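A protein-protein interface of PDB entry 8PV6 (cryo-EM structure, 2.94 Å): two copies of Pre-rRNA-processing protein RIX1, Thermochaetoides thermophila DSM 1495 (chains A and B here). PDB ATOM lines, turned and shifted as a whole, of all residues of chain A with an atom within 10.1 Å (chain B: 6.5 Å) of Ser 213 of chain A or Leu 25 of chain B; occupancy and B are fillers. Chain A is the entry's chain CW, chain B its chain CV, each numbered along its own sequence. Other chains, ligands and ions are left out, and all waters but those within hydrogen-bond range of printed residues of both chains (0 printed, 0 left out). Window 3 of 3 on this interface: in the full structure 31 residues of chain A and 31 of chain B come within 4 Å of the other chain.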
ATOM      1  N   PRO A 207     -30.365 -27.418  16.090  1.00  0.00           N
ATOM      2  CA  PRO A 207     -29.498 -27.356  14.895  1.00  0.00           C
ATOM      3  C   PRO A 207     -29.390 -28.660  14.119  1.00  0.00           C
ATOM      4  O   PRO A 207     -29.020 -28.636  12.939  1.00  0.00           O
ATOM      5  CB  PRO A 207     -28.138 -26.945  15.474  1.00  0.00           C
ATOM      6  CG  PRO A 207     -28.453 -26.268  16.735  1.00  0.00           C
ATOM      7  CD  PRO A 207     -29.589 -27.051  17.293  1.00  0.00           C
ATOM      8  N   ALA A 210     -32.417 -30.096  10.518  1.00  0.00           N
ATOM      9  CA  ALA A 210     -32.125 -29.898   9.101  1.00  0.00           C
ATOM     10  C   ALA A 210     -30.869 -29.045   8.966  1.00  0.00           C
ATOM     11  O   ALA A 210     -30.950 -27.847   8.662  1.00  0.00           O
ATOM     12  CB  ALA A 210     -33.305 -29.253   8.379  1.00  0.00           C
ATOM     13  N   PRO A 211     -29.692 -29.626   9.201  1.00  0.00           N
ATOM     14  CA  PRO A 211     -28.453 -28.848   9.092  1.00  0.00           C
ATOM     15  C   PRO A 211     -28.155 -28.477   7.650  1.00  0.00           C
ATOM     16  O   PRO A 211     -28.455 -29.226   6.719  1.00  0.00           O
ATOM     17  CB  PRO A 211     -27.385 -29.796   9.654  1.00  0.00           C
ATOM     18  CG  PRO A 211     -28.144 -30.896  10.333  1.00  0.00           C
ATOM     19  CD  PRO A 211     -29.418 -31.018   9.577  1.00  0.00           C
ATOM     20  N   THR A 212     -27.558 -27.305   7.476  1.00  0.00           N
ATOM     21  CA  THR A 212     -27.203 -26.781   6.167  1.00  0.00           C
ATOM     22  C   THR A 212     -25.705 -26.516   6.102  1.00  0.00           C
ATOM     23  O   THR A 212     -24.980 -26.639   7.092  1.00  0.00           O
ATOM     24  CB  THR A 212     -27.984 -25.497   5.868  1.00  0.00           C
ATOM     25  OG1 THR A 212     -27.804 -24.568   6.943  1.00  0.00           O
ATOM     26  CG2 THR A 212     -29.461 -25.802   5.730  1.00  0.00           C
ATOM     27  N   SER A 213     -25.242 -26.146   4.908  1.00  0.00           N
ATOM     28  CA  SER A 213     -23.851 -25.755   4.726  1.00  0.00           C
ATOM     29  C   SER A 213     -23.542 -24.384   5.308  1.00  0.00           C
ATOM     30  O   SER A 213     -22.364 -24.028   5.414  1.00  0.00           O
ATOM     31  CB  SER A 213     -23.487 -25.776   3.240  1.00  0.00           C
ATOM     32  OG  SER A 213     -24.311 -24.893   2.501  1.00  0.00           O
ATOM     33  N   SER A 214     -24.559 -23.614   5.685  1.00  0.00           N
ATOM     34  CA  SER A 214     -24.370 -22.311   6.304  1.00  0.00           C
ATOM     35  C   SER A 214     -24.194 -22.402   7.814  1.00  0.00           C
ATOM     36  O   SER A 214     -23.956 -21.378   8.461  1.00  0.00           O
ATOM     37  CB  SER A 214     -25.551 -21.396   5.976  1.00  0.00           C
ATOM     38  OG  SER A 214     -25.781 -21.342   4.579  1.00  0.00           O
ATOM     39  N   ASP A 215     -24.307 -23.600   8.386  1.00  0.00           N
ATOM     40  CA  ASP A 215     -24.067 -23.799   9.807  1.00  0.00           C
ATOM     41  C   ASP A 215     -22.601 -24.028  10.134  1.00  0.00           C
ATOM     42  O   ASP A 215     -22.208 -23.840  11.291  1.00  0.00           O
ATOM     43  CB  ASP A 215     -24.883 -24.991  10.323  1.00  0.00           C
ATOM     44  CG  ASP A 215     -26.376 -24.784  10.168  1.00  0.00           C
ATOM     45  OD1 ASP A 215     -26.788 -23.658   9.823  1.00  0.00           O
ATOM     46  OD2 ASP A 215     -27.137 -25.750  10.387  1.00  0.00           O
ATOM     47  N   ASN A 216     -21.803 -24.425   9.136  1.00  0.00           N
ATOM     48  CA  ASN A 216     -20.364 -24.682   9.258  1.00  0.00           C
ATOM     49  C   ASN A 216     -20.109 -25.751  10.329  1.00  0.00           C
ATOM     50  O   ASN A 216     -19.172 -25.667  11.127  1.00  0.00           O
ATOM     51  CB  ASN A 216     -19.607 -23.369   9.531  1.00  0.00           C
ATOM     52  CG  ASN A 216     -18.084 -23.498   9.435  1.00  0.00           C
ATOM     53  OD1 ASN A 216     -17.539 -24.571   9.181  1.00  0.00           O
ATOM     54  ND2 ASN A 216     -17.394 -22.381   9.636  1.00  0.00           N
ATOM     55  N   VAL A 217     -20.998 -26.741  10.395  1.00  0.00           N
ATOM     56  CA  VAL A 217     -20.874 -27.881  11.300  1.00  0.00           C
ATOM     57  C   VAL A 217     -21.229 -29.135  10.515  1.00  0.00           C
ATOM     58  O   VAL A 217     -22.265 -29.188   9.846  1.00  0.00           O
ATOM     59  CB  VAL A 217     -21.780 -27.741  12.547  1.00  0.00           C
ATOM     60  CG1 VAL A 217     -21.705 -28.991  13.406  1.00  0.00           C
ATOM     61  CG2 VAL A 217     -21.403 -26.523  13.387  1.00  0.00           C
ATOM     62  N   VAL A 218     -20.368 -30.146  10.588  1.00  0.00           N
ATOM     63  CA  VAL A 218     -20.612 -31.422   9.927  1.00  0.00           C
ATOM     64  C   VAL A 218     -21.407 -32.301  10.888  1.00  0.00           C
ATOM     65  O   VAL A 218     -20.866 -32.808  11.873  1.00  0.00           O
ATOM     66  CB  VAL A 218     -19.304 -32.097   9.505  1.00  0.00           C
ATOM     67  CG1 VAL A 218     -19.590 -33.433   8.838  1.00  0.00           C
ATOM     68  CG2 VAL A 218     -18.523 -31.187   8.574  1.00  0.00           C
ATOM     69  N   VAL A 219     -22.693 -32.481  10.601  1.00  0.00           N
ATOM     70  CA  VAL A 219     -23.589 -33.231  11.478  1.00  0.00           C
ATOM     71  C   VAL A 219     -23.787 -34.638  10.926  1.00  0.00           C
ATOM     72  O   VAL A 219     -24.151 -34.796   9.752  1.00  0.00           O
ATOM     73  CB  VAL A 219     -24.933 -32.507  11.643  1.00  0.00           C
ATOM     74  CG1 VAL A 219     -25.789 -33.211  12.678  1.00  0.00           C
ATOM     75  CG2 VAL A 219     -24.703 -31.059  12.035  1.00  0.00           C
ATOM     76  N   LYS A 224     -28.625 -36.773  13.103  1.00  0.00           N
ATOM     77  CA  LYS A 224     -29.786 -36.132  12.490  1.00  0.00           C
ATOM     78  C   LYS A 224     -31.049 -36.960  12.692  1.00  0.00           C
ATOM     79  O   LYS A 224     -32.080 -36.441  13.140  1.00  0.00           O
ATOM     80  CB  LYS A 224     -29.534 -35.896  11.002  1.00  0.00           C
ATOM     81  CG  LYS A 224     -28.488 -34.847  10.703  1.00  0.00           C
ATOM     82  CD  LYS A 224     -28.482 -34.473   9.234  1.00  0.00           C
ATOM     83  CE  LYS A 224     -28.071 -35.630   8.357  1.00  0.00           C
ATOM     84  NZ  LYS A 224     -27.887 -35.209   6.941  1.00  0.00           N
ATOM     85  N   PRO A 290     -31.167 -16.344  -2.038  1.00  0.00           N
ATOM     86  CA  PRO A 290     -32.279 -16.890  -1.252  1.00  0.00           C
ATOM     87  C   PRO A 290     -31.880 -17.091   0.203  1.00  0.00           C
ATOM     88  O   PRO A 290     -30.764 -17.516   0.508  1.00  0.00           O
ATOM     89  CB  PRO A 290     -32.585 -18.226  -1.941  1.00  0.00           C
ATOM     90  CG  PRO A 290     -31.383 -18.539  -2.752  1.00  0.00           C
ATOM     91  CD  PRO A 290     -30.786 -17.232  -3.147  1.00  0.00           C
ATOM     92  N   PRO A 301     -32.596 -22.975  12.448  1.00  0.00           N
ATOM     93  CA  PRO A 301     -31.490 -22.013  12.265  1.00  0.00           C
ATOM     94  C   PRO A 301     -31.396 -21.522  10.832  1.00  0.00           C
ATOM     95  O   PRO A 301     -31.727 -22.259   9.892  1.00  0.00           O
ATOM     96  CB  PRO A 301     -30.250 -22.830  12.648  1.00  0.00           C
ATOM     97  CG  PRO A 301     -30.746 -23.782  13.655  1.00  0.00           C
ATOM     98  CD  PRO A 301     -32.175 -24.109  13.295  1.00  0.00           C
ATOM     99  N   PRO A 302     -30.966 -20.275  10.629  1.00  0.00           N
ATOM    100  CA  PRO A 302     -31.058 -19.664   9.298  1.00  0.00           C
ATOM    101  C   PRO A 302     -30.079 -20.266   8.301  1.00  0.00           C
ATOM    102  O   PRO A 302     -29.090 -20.902   8.667  1.00  0.00           O
ATOM    103  CB  PRO A 302     -30.733 -18.190   9.565  1.00  0.00           C
ATOM    104  CG  PRO A 302     -30.971 -18.005  11.027  1.00  0.00           C
ATOM    105  CD  PRO A 302     -30.548 -19.296  11.643  1.00  0.00           C
ATOM    106  N   TRP A 303     -30.380 -20.054   7.023  1.00  0.00           N
ATOM    107  CA  TRP A 303     -29.547 -20.517   5.926  1.00  0.00           C
ATOM    108  C   TRP A 303     -29.448 -19.420   4.877  1.00  0.00           C
ATOM    109  O   TRP A 303     -30.308 -18.540   4.785  1.00  0.00           O
ATOM    110  CB  TRP A 303     -30.100 -21.803   5.299  1.00  0.00           C
ATOM    111  CG  TRP A 303     -31.507 -21.671   4.809  1.00  0.00           C
ATOM    112  CD1 TRP A 303     -32.641 -21.956   5.505  1.00  0.00           C
ATOM    113  CD2 TRP A 303     -31.932 -21.222   3.517  1.00  0.00           C
ATOM    114  NE1 TRP A 303     -33.747 -21.712   4.731  1.00  0.00           N
ATOM    115  CE2 TRP A 303     -33.338 -21.261   3.505  1.00  0.00           C
ATOM    116  CE3 TRP A 303     -31.261 -20.792   2.369  1.00  0.00           C
ATOM    117  CZ2 TRP A 303     -34.084 -20.885   2.393  1.00  0.00           C
ATOM    118  CZ3 TRP A 303     -32.005 -20.417   1.269  1.00  0.00           C
ATOM    119  CH2 TRP A 303     -33.400 -20.469   1.287  1.00  0.00           C
ATOM    120  N   SER A 304     -28.382 -19.480   4.083  1.00  0.00           N
ATOM    121  CA  SER A 304     -28.191 -18.541   2.991  1.00  0.00           C
ATOM    122  C   SER A 304     -27.592 -19.278   1.805  1.00  0.00           C
ATOM    123  O   SER A 304     -26.648 -20.058   1.953  1.00  0.00           O
ATOM    124  CB  SER A 304     -27.289 -17.371   3.400  1.00  0.00           C
ATOM    125  OG  SER A 304     -27.061 -16.500   2.307  1.00  0.00           O
ATOM    126  N   GLY A 305     -28.146 -19.022   0.629  1.00  0.00           N
ATOM    127  CA  GLY A 305     -27.704 -19.680  -0.579  1.00  0.00           C
ATOM    128  C   GLY A 305     -28.680 -20.751  -1.041  1.00  0.00           C
ATOM    129  O   GLY A 305     -29.392 -21.380  -0.251  1.00  0.00           O
ATOM    130  N   LEU A 306     -28.700 -20.958  -2.361  1.00  0.00           N
ATOM    131  CA  LEU A 306     -29.610 -21.932  -2.957  1.00  0.00           C
ATOM    132  C   LEU A 306     -29.268 -23.353  -2.535  1.00  0.00           C
ATOM    133  O   LEU A 306     -30.166 -24.174  -2.315  1.00  0.00           O
ATOM    134  CB  LEU A 306     -29.579 -21.809  -4.478  1.00  0.00           C
ATOM    135  CG  LEU A 306     -30.758 -22.436  -5.218  1.00  0.00           C
ATOM    136  CD1 LEU A 306     -32.002 -21.594  -5.023  1.00  0.00           C
ATOM    137  CD2 LEU A 306     -30.426 -22.579  -6.685  1.00  0.00           C
ATOM    138  N   GLN A 307     -27.974 -23.663  -2.418  1.00  0.00           N
ATOM    139  CA  GLN A 307     -27.567 -24.998  -1.994  1.00  0.00           C
ATOM    140  C   GLN A 307     -27.983 -25.262  -0.551  1.00  0.00           C
ATOM    141  O   GLN A 307     -28.463 -26.353  -0.218  1.00  0.00           O
ATOM    142  CB  GLN A 307     -26.056 -25.160  -2.165  1.00  0.00           C
ATOM    143  CG  GLN A 307     -25.512 -26.486  -1.665  1.00  0.00           C
ATOM    144  CD  GLN A 307     -25.912 -27.654  -2.551  1.00  0.00           C
ATOM    145  OE1 GLN A 307     -26.325 -27.472  -3.696  1.00  0.00           O
ATOM    146  NE2 GLN A 307     -25.804 -28.863  -2.015  1.00  0.00           N
ATOM    147  N   ALA A 308     -27.820 -24.259   0.317  1.00  0.00           N
ATOM    148  CA  ALA A 308     -28.269 -24.385   1.698  1.00  0.00           C
ATOM    149  C   ALA A 308     -29.782 -24.528   1.783  1.00  0.00           C
ATOM    150  O   ALA A 308     -30.285 -25.290   2.614  1.00  0.00           O
ATOM    151  CB  ALA A 308     -27.804 -23.183   2.515  1.00  0.00           C
ATOM    152  N   GLY A 309     -30.517 -23.814   0.927  1.00  0.00           N
ATOM    153  CA  GLY A 309     -31.959 -24.001   0.873  1.00  0.00           C
ATOM    154  C   GLY A 309     -32.348 -25.399   0.432  1.00  0.00           C
ATOM    155  O   GLY A 309     -33.307 -25.979   0.952  1.00  0.00           O
ATOM    156  N   ALA A 310     -31.608 -25.959  -0.527  1.00  0.00           N
ATOM    157  CA  ALA A 310     -31.835 -27.335  -0.952  1.00  0.00           C
ATOM    158  C   ALA A 310     -31.583 -28.340   0.164  1.00  0.00           C
ATOM    159  O   ALA A 310     -32.380 -29.270   0.332  1.00  0.00           O
ATOM    160  CB  ALA A 310     -30.951 -27.671  -2.151  1.00  0.00           C
ATOM    161  N   GLU A 311     -30.501 -28.170   0.930  1.00  0.00           N
ATOM    162  CA  GLU A 311     -30.268 -29.070   2.061  1.00  0.00           C
ATOM    163  C   GLU A 311     -31.316 -28.892   3.154  1.00  0.00           C
ATOM    164  O   GLU A 311     -31.697 -29.867   3.807  1.00  0.00           O
ATOM    165  CB  GLU A 311     -28.863 -28.899   2.637  1.00  0.00           C
ATOM    166  CG  GLU A 311     -27.750 -28.803   1.622  1.00  0.00           C
ATOM    167  CD  GLU A 311     -26.390 -28.676   2.272  1.00  0.00           C
ATOM    168  OE1 GLU A 311     -26.128 -29.409   3.247  1.00  0.00           O
ATOM    169  OE2 GLU A 311     -25.581 -27.847   1.806  1.00  0.00           O
ATOM    170  N   ARG A 312     -31.788 -27.662   3.376  1.00  0.00           N
ATOM    171  CA  ARG A 312     -32.852 -27.444   4.355  1.00  0.00           C
ATOM    172  C   ARG A 312     -34.139 -28.146   3.935  1.00  0.00           C
ATOM    173  O   ARG A 312     -34.811 -28.784   4.757  1.00  0.00           O
ATOM    174  CB  ARG A 312     -33.099 -25.949   4.544  1.00  0.00           C
ATOM    175  CG  ARG A 312     -34.256 -25.637   5.467  1.00  0.00           C
ATOM    176  CD  ARG A 312     -33.854 -25.778   6.918  1.00  0.00           C
ATOM    177  NE  ARG A 312     -32.729 -24.915   7.253  1.00  0.00           N
ATOM    178  CZ  ARG A 312     -32.063 -24.972   8.397  1.00  0.00           C
ATOM    179  NH1 ARG A 312     -32.373 -25.851   9.333  1.00  0.00           N
ATOM    180  NH2 ARG A 312     -31.055 -24.129   8.603  1.00  0.00           N
ATOM    181  N   LEU A 313     -34.491 -28.050   2.650  1.00  0.00           N
ATOM    182  CA  LEU A 313     -35.691 -28.715   2.155  1.00  0.00           C
ATOM    183  C   LEU A 313     -35.553 -30.233   2.221  1.00  0.00           C
ATOM    184  O   LEU A 313     -36.509 -30.936   2.570  1.00  0.00           O
ATOM    185  CB  LEU A 313     -35.984 -28.260   0.727  1.00  0.00           C
ATOM    186  CG  LEU A 313     -37.250 -28.796   0.062  1.00  0.00           C
ATOM    187  CD1 LEU A 313     -38.461 -28.548   0.943  1.00  0.00           C
ATOM    188  CD2 LEU A 313     -37.435 -28.153  -1.296  1.00  0.00           C
ATOM    189  N   GLU A 373     -27.399 -24.046 -10.643  1.00  0.00           N
ATOM    190  CA  GLU A 373     -27.372 -24.622  -9.302  1.00  0.00           C
ATOM    191  C   GLU A 373     -28.696 -25.289  -8.946  1.00  0.00           C
ATOM    192  O   GLU A 373     -28.706 -26.347  -8.306  1.00  0.00           O
ATOM    193  CB  GLU A 373     -27.026 -23.542  -8.278  1.00  0.00           C
ATOM    194  CG  GLU A 373     -26.578 -24.082  -6.934  1.00  0.00           C
ATOM    195  CD  GLU A 373     -25.815 -23.055  -6.123  1.00  0.00           C
ATOM    196  OE1 GLU A 373     -25.360 -22.050  -6.709  1.00  0.00           O
ATOM    197  OE2 GLU A 373     -25.670 -23.251  -4.897  1.00  0.00           O
ATOM    198  N   ARG B  13     -17.790 -23.187  -7.080  1.00  0.00           N
ATOM    199  CA  ARG B  13     -17.571 -23.380  -5.650  1.00  0.00           C
ATOM    200  C   ARG B  13     -16.090 -23.545  -5.333  1.00  0.00           C
ATOM    201  O   ARG B  13     -15.620 -23.096  -4.283  1.00  0.00           O
ATOM    202  CB  ARG B  13     -18.374 -24.577  -5.139  1.00  0.00           C
ATOM    203  CG  ARG B  13     -19.883 -24.402  -5.239  1.00  0.00           C
ATOM    204  CD  ARG B  13     -20.607 -25.020  -4.043  1.00  0.00           C
ATOM    205  NE  ARG B  13     -20.692 -24.135  -2.883  1.00  0.00           N
ATOM    206  CZ  ARG B  13     -21.395 -23.009  -2.821  1.00  0.00           C
ATOM    207  NH1 ARG B  13     -22.171 -22.614  -3.818  1.00  0.00           N
ATOM    208  NH2 ARG B  13     -21.337 -22.272  -1.715  1.00  0.00           N
ATOM    209  N   THR B  17     -14.912 -20.733  -2.787  1.00  0.00           N
ATOM    210  CA  THR B  17     -14.783 -21.235  -1.427  1.00  0.00           C
ATOM    211  C   THR B  17     -13.331 -21.159  -0.954  1.00  0.00           C
ATOM    212  O   THR B  17     -12.415 -21.500  -1.707  1.00  0.00           O
ATOM    213  CB  THR B  17     -15.282 -22.679  -1.357  1.00  0.00           C
ATOM    214  OG1 THR B  17     -16.585 -22.764  -1.949  1.00  0.00           O
ATOM    215  CG2 THR B  17     -15.363 -23.160   0.079  1.00  0.00           C
ATOM    216  N   SER B  21     -12.761 -24.342   4.464  1.00  0.00           N
ATOM    217  CA  SER B  21     -14.133 -24.822   4.571  1.00  0.00           C
ATOM    218  C   SER B  21     -14.514 -25.796   3.464  1.00  0.00           C
ATOM    219  O   SER B  21     -15.674 -26.214   3.400  1.00  0.00           O
ATOM    220  CB  SER B  21     -15.104 -23.639   4.580  1.00  0.00           C
ATOM    221  OG  SER B  21     -15.058 -22.927   3.358  1.00  0.00           O
ATOM    222  N   LEU B  22     -13.580 -26.148   2.586  1.00  0.00           N
ATOM    223  CA  LEU B  22     -13.771 -27.172   1.563  1.00  0.00           C
ATOM    224  C   LEU B  22     -14.119 -28.563   2.111  1.00  0.00           C
ATOM    225  O   LEU B  22     -14.914 -29.263   1.465  1.00  0.00           O
ATOM    226  CB  LEU B  22     -12.536 -27.251   0.659  1.00  0.00           C
ATOM    227  CG  LEU B  22     -12.440 -26.165  -0.412  1.00  0.00           C
ATOM    228  CD1 LEU B  22     -11.143 -26.292  -1.193  1.00  0.00           C
ATOM    229  CD2 LEU B  22     -13.641 -26.228  -1.342  1.00  0.00           C
ATOM    230  N   PRO B  23     -13.542 -29.041   3.238  1.00  0.00           N
ATOM    231  CA  PRO B  23     -14.039 -30.317   3.793  1.00  0.00           C
ATOM    232  C   PRO B  23     -15.509 -30.311   4.187  1.00  0.00           C
ATOM    233  O   PRO B  23     -16.135 -31.376   4.183  1.00  0.00           O
ATOM    234  CB  PRO B  23     -13.124 -30.549   5.001  1.00  0.00           C
ATOM    235  CG  PRO B  23     -11.865 -29.918   4.617  1.00  0.00           C
ATOM    236  CD  PRO B  23     -12.259 -28.679   3.881  1.00  0.00           C
ATOM    237  N   ARG B  24     -16.080 -29.156   4.537  1.00  0.00           N
ATOM    238  CA  ARG B  24     -17.531 -29.072   4.670  1.00  0.00           C
ATOM    239  C   ARG B  24     -18.252 -29.348   3.360  1.00  0.00           C
ATOM    240  O   ARG B  24     -19.293 -30.012   3.368  1.00  0.00           O
ATOM    241  CB  ARG B  24     -17.957 -27.695   5.190  1.00  0.00           C
ATOM    242  CG  ARG B  24     -17.761 -27.430   6.675  1.00  0.00           C
ATOM    243  CD  ARG B  24     -16.371 -26.957   7.035  1.00  0.00           C
ATOM    244  NE  ARG B  24     -16.342 -26.501   8.417  1.00  0.00           N
ATOM    245  CZ  ARG B  24     -16.012 -27.264   9.449  1.00  0.00           C
ATOM    246  NH1 ARG B  24     -15.761 -28.553   9.302  1.00  0.00           N
ATOM    247  NH2 ARG B  24     -15.958 -26.724  10.663  1.00  0.00           N
ATOM    248  N   LEU B  25     -17.726 -28.863   2.237  1.00  0.00           N
ATOM    249  CA  LEU B  25     -18.428 -28.946   0.965  1.00  0.00           C
ATOM    250  C   LEU B  25     -18.019 -30.154   0.134  1.00  0.00           C
ATOM    251  O   LEU B  25     -18.500 -30.299  -0.996  1.00  0.00           O
ATOM    252  CB  LEU B  25     -18.205 -27.664   0.160  1.00  0.00           C
ATOM    253  CG  LEU B  25     -18.815 -26.407   0.787  1.00  0.00           C
ATOM    254  CD1 LEU B  25     -18.433 -25.171  -0.006  1.00  0.00           C
ATOM    255  CD2 LEU B  25     -20.326 -26.514   0.941  1.00  0.00           C
ATOM    256  N   CYS B  26     -17.136 -31.002   0.657  1.00  0.00           N
ATOM    257  CA  CYS B  26     -16.802 -32.263  -0.008  1.00  0.00           C
ATOM    258  C   CYS B  26     -17.981 -33.193  -0.318  1.00  0.00           C
ATOM    259  O   CYS B  26     -17.930 -33.844  -1.375  1.00  0.00           O
ATOM    260  CB  CYS B  26     -15.741 -33.016   0.809  1.00  0.00           C
ATOM    261  SG  CYS B  26     -14.078 -32.316   0.717  1.00  0.00           S
ATOM    262  N   PRO B  27     -19.014 -33.365   0.537  1.00  0.00           N
ATOM    263  CA  PRO B  27     -20.132 -34.249   0.130  1.00  0.00           C
ATOM    264  C   PRO B  27     -20.848 -33.838  -1.149  1.00  0.00           C
ATOM    265  O   PRO B  27     -21.246 -34.709  -1.934  1.00  0.00           O
ATOM    266  CB  PRO B  27     -21.075 -34.188   1.338  1.00  0.00           C
ATOM    267  CG  PRO B  27     -20.210 -33.928   2.473  1.00  0.00           C
ATOM    268  CD  PRO B  27     -19.118 -33.036   1.975  1.00  0.00           C
ATOM    269  N   LEU B  28     -21.029 -32.539  -1.386  1.00  0.00           N
ATOM    270  CA  LEU B  28     -21.758 -32.114  -2.578  1.00  0.00           C
ATOM    271  C   LEU B  28     -20.843 -32.029  -3.794  1.00  0.00           C
ATOM    272  O   LEU B  28     -21.278 -32.289  -4.926  1.00  0.00           O
ATOM    273  CB  LEU B  28     -22.466 -30.783  -2.308  1.00  0.00           C
ATOM    274  CG  LEU B  28     -21.700 -29.518  -1.905  1.00  0.00           C
ATOM    275  CD1 LEU B  28     -21.214 -28.690  -3.096  1.00  0.00           C
ATOM    276  CD2 LEU B  28     -22.571 -28.679  -0.989  1.00  0.00           C
ATOM    277  N   LEU B  29     -19.576 -31.655  -3.582  1.00  0.00           N
ATOM    278  CA  LEU B  29     -18.615 -31.601  -4.679  1.00  0.00           C
ATOM    279  C   LEU B  29     -18.394 -32.980  -5.281  1.00  0.00           C
ATOM    280  O   LEU B  29     -18.331 -33.130  -6.507  1.00  0.00           O
ATOM    281  CB  LEU B  29     -17.291 -31.016  -4.191  1.00  0.00           C
ATOM    282  CG  LEU B  29     -17.242 -29.504  -3.975  1.00  0.00           C
ATOM    283  CD1 LEU B  29     -15.969 -29.114  -3.243  1.00  0.00           C
ATOM    284  CD2 LEU B  29     -17.346 -28.772  -5.302  1.00  0.00           C
ATOM    285  N   ILE B  30     -18.291 -34.002  -4.429  1.00  0.00           N
ATOM    286  CA  ILE B  30     -18.153 -35.371  -4.908  1.00  0.00           C
ATOM    287  C   ILE B  30     -19.392 -35.803  -5.682  1.00  0.00           C
ATOM    288  O   ILE B  30     -19.273 -36.439  -6.732  1.00  0.00           O
ATOM    289  CB  ILE B  30     -17.835 -36.308  -3.728  1.00  0.00           C
ATOM    290  CG1 ILE B  30     -16.371 -36.139  -3.320  1.00  0.00           C
ATOM    291  CG2 ILE B  30     -18.138 -37.763  -4.059  1.00  0.00           C
ATOM    292  CD1 ILE B  30     -15.901 -37.141  -2.305  1.00  0.00           C
ATOM    293  N   THR B  80      -9.432 -32.366   0.346  1.00  0.00           N
ATOM    294  CA  THR B  80     -10.379 -32.186  -0.749  1.00  0.00           C
ATOM    295  C   THR B  80      -9.802 -32.703  -2.060  1.00  0.00           C
ATOM    296  O   THR B  80     -10.528 -33.273  -2.887  1.00  0.00           O
ATOM    297  CB  THR B  80     -10.759 -30.710  -0.869  1.00  0.00           C
ATOM    298  OG1 THR B  80     -11.107 -30.205   0.425  1.00  0.00           O
ATOM    299  CG2 THR B  80     -11.943 -30.532  -1.803  1.00  0.00           C
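Among the printed residues, pairs that only touch across the chains: Ser 213 of chain A with Leu 25 of chain B (3.98 Å), Val 218 of chain A with Arg 24 of chain B (3.9 Å) and Gln 307 of chain A with Leu 28 of chain B (3.4 Å).
Pro 211 of chain A touches none of the printed residues of chain B.
Ser 213 of chain A touches just one residue of chain B: Leu 25 (3.98 Å).
Of the printed residues of chain B, Asn 216 of chain A touches Arg 24.
Of the printed residues of chain B, Val 218 of chain A touches Arg 24.
Of the printed residues of chain A, Arg 13 of chain B touches Glu 373.
Of the printed residues of chain A, Arg 24 of chain B touches Asn 216 and Val 218.
No residue of chain A comes within 4 Å of Pro 27 of chain B.
Ile 30 of chain B touches none of the printed residues of chain A.
The nearest residue of chain A that does not touch Leu 25 of chain B is Glu 311 of chain A (5.5 Å).
No position is printed for both chains.
Of the 27 printed residues of chain A, 5 touch a printed residue of chain B.
Hydrophobic or aromatic side chains of chain B that line the printed part of chain A: Leu 25 and Leu 28.
Among the printed residues, Asp or Glu carboxylates within 4 Å of a Lys or Arg side-chain nitrogen of the other chain: Glu 373 of chain A with Arg 13 of chain B.
The side-chain hydroxyl (OG1) of Thr 17 of chain B is in hydrogen-bond range of the backbone carbonyl oxygen (O) of Arg 13 of chain B.
The side-chain hydroxyl (OG) of Ser 213 of chain A sits close to the side-chain carboxylate (OE2) of Glu 311 of chain A (3.3 Å).
N of Gln 307 of chain A lies close to OE2 of Glu 373 of chain A, at 3.4 Å.
The guanidinium group (NH1) of Arg 13 of chain B is in salt-bridge range of the side-chain carboxylate (OE2) of Glu 373 of chain A (3.7 Å).
The guanidinium group (NH2) of Arg 24 of chain B sits at hydrogen-bond distance from the side-chain amide oxygen (OD1) of Asn 216 of chain A (3.1 Å).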
